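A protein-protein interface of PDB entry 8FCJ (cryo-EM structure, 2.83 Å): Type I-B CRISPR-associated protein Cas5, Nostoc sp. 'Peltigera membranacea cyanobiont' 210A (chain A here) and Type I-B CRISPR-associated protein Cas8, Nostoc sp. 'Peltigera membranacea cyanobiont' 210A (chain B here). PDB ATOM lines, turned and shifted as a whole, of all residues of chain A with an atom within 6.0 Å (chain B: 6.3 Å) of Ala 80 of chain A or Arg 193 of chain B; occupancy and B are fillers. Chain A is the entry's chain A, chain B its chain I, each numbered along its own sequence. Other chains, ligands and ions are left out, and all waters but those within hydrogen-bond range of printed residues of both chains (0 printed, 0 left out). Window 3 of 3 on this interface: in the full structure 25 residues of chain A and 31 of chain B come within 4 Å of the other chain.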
ATOM      1  N   PHE A  77     -18.860 -27.764  22.844  1.00  0.00           N
ATOM      2  CA  PHE A  77     -19.630 -28.657  21.982  1.00  0.00           C
ATOM      3  C   PHE A  77     -20.681 -27.827  21.252  1.00  0.00           C
ATOM      4  O   PHE A  77     -21.849 -27.771  21.633  1.00  0.00           O
ATOM      5  CB  PHE A  77     -20.258 -29.781  22.795  1.00  0.00           C
ATOM      6  CG  PHE A  77     -19.292 -30.486  23.700  1.00  0.00           C
ATOM      7  CD1 PHE A  77     -18.315 -31.312  23.179  1.00  0.00           C
ATOM      8  CD2 PHE A  77     -19.363 -30.324  25.071  1.00  0.00           C
ATOM      9  CE1 PHE A  77     -17.426 -31.961  24.007  1.00  0.00           C
ATOM     10  CE2 PHE A  77     -18.474 -30.970  25.904  1.00  0.00           C
ATOM     11  CZ  PHE A  77     -17.507 -31.790  25.371  1.00  0.00           C
ATOM     12  N   LYS A  78     -20.246 -27.167  20.181  1.00  0.00           N
ATOM     13  CA  LYS A  78     -21.135 -26.365  19.351  1.00  0.00           C
ATOM     14  C   LYS A  78     -21.484 -27.039  18.033  1.00  0.00           C
ATOM     15  O   LYS A  78     -22.638 -26.983  17.602  1.00  0.00           O
ATOM     16  CB  LYS A  78     -20.511 -24.997  19.067  1.00  0.00           C
ATOM     17  CG  LYS A  78     -21.359 -24.117  18.167  1.00  0.00           C
ATOM     18  CD  LYS A  78     -20.939 -22.664  18.248  1.00  0.00           C
ATOM     19  CE  LYS A  78     -21.873 -21.784  17.441  1.00  0.00           C
ATOM     20  NZ  LYS A  78     -21.673 -20.345  17.745  1.00  0.00           N
ATOM     21  N   ASN A  79     -20.516 -27.680  17.388  1.00  0.00           N
ATOM     22  CA  ASN A  79     -20.735 -28.360  16.122  1.00  0.00           C
ATOM     23  C   ASN A  79     -20.441 -29.844  16.278  1.00  0.00           C
ATOM     24  O   ASN A  79     -19.621 -30.249  17.106  1.00  0.00           O
ATOM     25  CB  ASN A  79     -19.858 -27.772  15.015  1.00  0.00           C
ATOM     26  CG  ASN A  79     -20.449 -27.975  13.638  1.00  0.00           C
ATOM     27  OD1 ASN A  79     -19.734 -28.252  12.678  1.00  0.00           O
ATOM     28  ND2 ASN A  79     -21.764 -27.841  13.536  1.00  0.00           N
ATOM     29  N   ALA A  80     -21.130 -30.655  15.473  1.00  0.00           N
ATOM     30  CA  ALA A  80     -20.913 -32.097  15.519  1.00  0.00           C
ATOM     31  C   ALA A  80     -19.491 -32.453  15.109  1.00  0.00           C
ATOM     32  O   ALA A  80     -18.874 -33.351  15.693  1.00  0.00           O
ATOM     33  CB  ALA A  80     -21.925 -32.808  14.623  1.00  0.00           C
ATOM     34  N   ASP A  81     -18.955 -31.765  14.105  1.00  0.00           N
ATOM     35  CA  ASP A  81     -17.586 -32.008  13.677  1.00  0.00           C
ATOM     36  C   ASP A  81     -16.613 -31.491  14.728  1.00  0.00           C
ATOM     37  O   ASP A  81     -16.714 -30.344  15.173  1.00  0.00           O
ATOM     38  CB  ASP A  81     -17.326 -31.331  12.333  1.00  0.00           C
ATOM     39  CG  ASP A  81     -16.049 -31.813  11.669  1.00  0.00           C
ATOM     40  OD1 ASP A  81     -15.217 -32.450  12.347  1.00  0.00           O
ATOM     41  OD2 ASP A  81     -15.881 -31.560  10.457  1.00  0.00           O
ATOM     42  N   PHE A  82     -15.667 -32.343  15.126  1.00  0.00           N
ATOM     43  CA  PHE A  82     -14.669 -31.930  16.105  1.00  0.00           C
ATOM     44  C   PHE A  82     -13.743 -30.865  15.533  1.00  0.00           C
ATOM     45  O   PHE A  82     -13.333 -29.942  16.244  1.00  0.00           O
ATOM     46  CB  PHE A  82     -13.868 -33.143  16.576  1.00  0.00           C
ATOM     47  CG  PHE A  82     -12.904 -32.842  17.687  1.00  0.00           C
ATOM     48  CD1 PHE A  82     -11.608 -32.446  17.412  1.00  0.00           C
ATOM     49  CD2 PHE A  82     -13.294 -32.966  19.008  1.00  0.00           C
ATOM     50  CE1 PHE A  82     -10.723 -32.174  18.433  1.00  0.00           C
ATOM     51  CE2 PHE A  82     -12.411 -32.695  20.032  1.00  0.00           C
ATOM     52  CZ  PHE A  82     -11.125 -32.299  19.743  1.00  0.00           C
ATOM     53  N   ASN A  87     -15.917 -24.822  17.219  1.00  0.00           N
ATOM     54  CA  ASN A  87     -15.748 -25.497  18.498  1.00  0.00           C
ATOM     55  C   ASN A  87     -14.694 -24.851  19.386  1.00  0.00           C
ATOM     56  O   ASN A  87     -14.557 -25.257  20.543  1.00  0.00           O
ATOM     57  CB  ASN A  87     -15.390 -26.966  18.270  1.00  0.00           C
ATOM     58  CG  ASN A  87     -16.534 -27.755  17.674  1.00  0.00           C
ATOM     59  OD1 ASN A  87     -17.687 -27.337  17.736  1.00  0.00           O
ATOM     60  ND2 ASN A  87     -16.219 -28.903  17.089  1.00  0.00           N
ATOM     61  N   VAL B 189     -25.025 -20.063  26.912  1.00  0.00           N
ATOM     62  CA  VAL B 189     -25.024 -21.517  26.791  1.00  0.00           C
ATOM     63  C   VAL B 189     -23.711 -21.904  26.122  1.00  0.00           C
ATOM     64  O   VAL B 189     -23.531 -21.688  24.922  1.00  0.00           O
ATOM     65  CB  VAL B 189     -26.230 -22.021  25.993  1.00  0.00           C
ATOM     66  CG1 VAL B 189     -26.246 -23.536  25.966  1.00  0.00           C
ATOM     67  CG2 VAL B 189     -27.515 -21.486  26.591  1.00  0.00           C
ATOM     68  N   HIS B 191     -22.269 -24.823  25.421  1.00  0.00           N
ATOM     69  CA  HIS B 191     -22.357 -25.900  24.443  1.00  0.00           C
ATOM     70  C   HIS B 191     -23.708 -25.805  23.749  1.00  0.00           C
ATOM     71  O   HIS B 191     -24.743 -26.112  24.348  1.00  0.00           O
ATOM     72  CB  HIS B 191     -22.165 -27.253  25.119  1.00  0.00           C
ATOM     73  CG  HIS B 191     -21.054 -27.269  26.122  1.00  0.00           C
ATOM     74  ND1 HIS B 191     -19.730 -27.140  25.765  1.00  0.00           N
ATOM     75  CD2 HIS B 191     -21.071 -27.391  27.469  1.00  0.00           C
ATOM     76  CE1 HIS B 191     -18.977 -27.187  26.849  1.00  0.00           C
ATOM     77  NE2 HIS B 191     -19.766 -27.338  27.898  1.00  0.00           N
ATOM     78  N   ALA B 192     -23.695 -25.380  22.484  1.00  0.00           N
ATOM     79  CA  ALA B 192     -24.935 -25.206  21.741  1.00  0.00           C
ATOM     80  C   ALA B 192     -25.649 -26.524  21.480  1.00  0.00           C
ATOM     81  O   ALA B 192     -26.870 -26.523  21.295  1.00  0.00           O
ATOM     82  CB  ALA B 192     -24.659 -24.496  20.416  1.00  0.00           C
ATOM     83  N   ARG B 193     -24.925 -27.642  21.461  1.00  0.00           N
ATOM     84  CA  ARG B 193     -25.553 -28.937  21.233  1.00  0.00           C
ATOM     85  C   ARG B 193     -26.357 -29.419  22.432  1.00  0.00           C
ATOM     86  O   ARG B 193     -27.081 -30.413  22.311  1.00  0.00           O
ATOM     87  CB  ARG B 193     -24.492 -29.973  20.866  1.00  0.00           C
ATOM     88  CG  ARG B 193     -23.691 -29.613  19.630  1.00  0.00           C
ATOM     89  CD  ARG B 193     -22.535 -30.572  19.417  1.00  0.00           C
ATOM     90  NE  ARG B 193     -22.990 -31.897  19.018  1.00  0.00           N
ATOM     91  CZ  ARG B 193     -22.227 -32.980  19.017  1.00  0.00           C
ATOM     92  NH1 ARG B 193     -20.960 -32.933  19.395  1.00  0.00           N
ATOM     93  NH2 ARG B 193     -22.746 -34.141  18.627  1.00  0.00           N
ATOM     94  N   THR B 194     -26.249 -28.750  23.574  1.00  0.00           N
ATOM     95  CA  THR B 194     -27.018 -29.064  24.772  1.00  0.00           C
ATOM     96  C   THR B 194     -27.936 -27.905  25.135  1.00  0.00           C
ATOM     97  O   THR B 194     -28.049 -27.517  26.299  1.00  0.00           O
ATOM     98  CB  THR B 194     -26.097 -29.396  25.942  1.00  0.00           C
ATOM     99  OG1 THR B 194     -25.385 -28.219  26.336  1.00  0.00           O
ATOM    100  CG2 THR B 194     -25.102 -30.465  25.548  1.00  0.00           C
ATOM    101  N   GLN B 195     -28.601 -27.331  24.129  1.00  0.00           N
ATOM    102  CA  GLN B 195     -29.407 -26.137  24.355  1.00  0.00           C
ATOM    103  C   GLN B 195     -30.594 -26.414  25.270  1.00  0.00           C
ATOM    104  O   GLN B 195     -31.035 -25.517  25.996  1.00  0.00           O
ATOM    105  CB  GLN B 195     -29.885 -25.565  23.018  1.00  0.00           C
ATOM    106  CG  GLN B 195     -30.968 -26.380  22.317  1.00  0.00           C
ATOM    107  CD  GLN B 195     -30.437 -27.635  21.647  1.00  0.00           C
ATOM    108  OE1 GLN B 195     -29.262 -27.975  21.775  1.00  0.00           O
ATOM    109  NE2 GLN B 195     -31.308 -28.333  20.926  1.00  0.00           N
ATOM    110  N   ASN B 196     -31.125 -27.636  25.251  1.00  0.00           N
ATOM    111  CA  ASN B 196     -32.297 -27.934  26.066  1.00  0.00           C
ATOM    112  C   ASN B 196     -31.943 -28.024  27.544  1.00  0.00           C
ATOM    113  O   ASN B 196     -32.673 -27.504  28.395  1.00  0.00           O
ATOM    114  CB  ASN B 196     -32.949 -29.233  25.593  1.00  0.00           C
ATOM    115  CG  ASN B 196     -32.833 -29.430  24.097  1.00  0.00           C
ATOM    116  OD1 ASN B 196     -31.743 -29.656  23.572  1.00  0.00           O
ATOM    117  ND2 ASN B 196     -33.961 -29.345  23.400  1.00  0.00           N
ATOM    118  N   THR B 198     -28.436 -27.688  29.335  1.00  0.00           N
ATOM    119  CA  THR B 198     -27.445 -26.803  29.949  1.00  0.00           C
ATOM    120  C   THR B 198     -27.853 -25.345  29.740  1.00  0.00           C
ATOM    121  O   THR B 198     -27.250 -24.588  28.978  1.00  0.00           O
ATOM    122  CB  THR B 198     -26.059 -27.077  29.387  1.00  0.00           C
ATOM    123  OG1 THR B 198     -26.039 -26.764  27.989  1.00  0.00           O
ATOM    124  CG2 THR B 198     -25.692 -28.538  29.577  1.00  0.00           C
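Of the 7 printed residues of chain A, 4 touch a printed residue of chain B. Printed residues of chain A that touch a printed residue of chain B: Phe 77, Lys 78, Asn 79 and Ala 80. Hydrophobic or aromatic side chains of chain A within 4 Å of the printed part of chain B: Phe 77. Among the printed residues, 6 pairs touch across the chains. Among the printed residues, no Asp or Glu carboxylate lies within 4 Å of a Lys or Arg side-chain nitrogen of the other chain.
O of Phe 77 of chain A sits at hydrogen-bond distance from N of Ala 192 of chain B (3.1 Å). The backbone carbonyl oxygen (O) of Phe 77 of chain A sits at hydrogen-bond distance from the backbone NH (N) of Arg 193 of chain B. ND1 of His 191 of chain B sits at hydrogen-bond distance from N of Phe 77 of chain A (3.1 Å).
Among the printed residues, pairs that only touch across the chains: Lys 78 of chain A with Arg 193 of chain B (3.5 Å), Asn 79 of chain A with Arg 193 of chain B (3.7 Å) and Ala 80 of chain A with Arg 193 of chain B (3.8 Å).
The backbone carbonyl oxygen (O) of Ala 192 of chain B sits close to the side-chain amide oxygen (OE1) of Gln 195 of chain B, 2.8 Å away. The side-chain hydroxyl (OG1) of Thr 194 of chain B sits at hydrogen-bond distance from the backbone carbonyl oxygen (O) of His 191 of chain B, 3.0 Å away. O of Arg 193 of chain B sits close to OE1 of Gln 195 of chain B (3.3 Å). The backbone NH of Asn 79 of chain A is in hydrogen-bond range of the side-chain amide oxygen of Asn 87 of chain A, at 2.9 Å.
Printed residues of chain B within 4 Å of Phe 77 of chain A: His 191, Ala 192 and Arg 193. Printed residues of chain B within 4 Å of Lys 78 of chain A: Arg 193 (3.5 Å). Of the printed residues of chain B, Asn 79 of chain A touches Arg 193 (3.7 Å). Ala 80 of chain A touches just one residue of chain B: Arg 193 (3.8 Å). Val 189 of chain B touches none of the printed residues of chain A. Arg 193 of chain B touches four residues of chain A. The nearest residue of chain A that does not touch Arg 193 of chain B is Asp 81 of chain A (5.8 Å). The nearest printed residue of chain B that does not touch Phe 77 of chain A is Thr 194 of chain B (4.9 Å).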
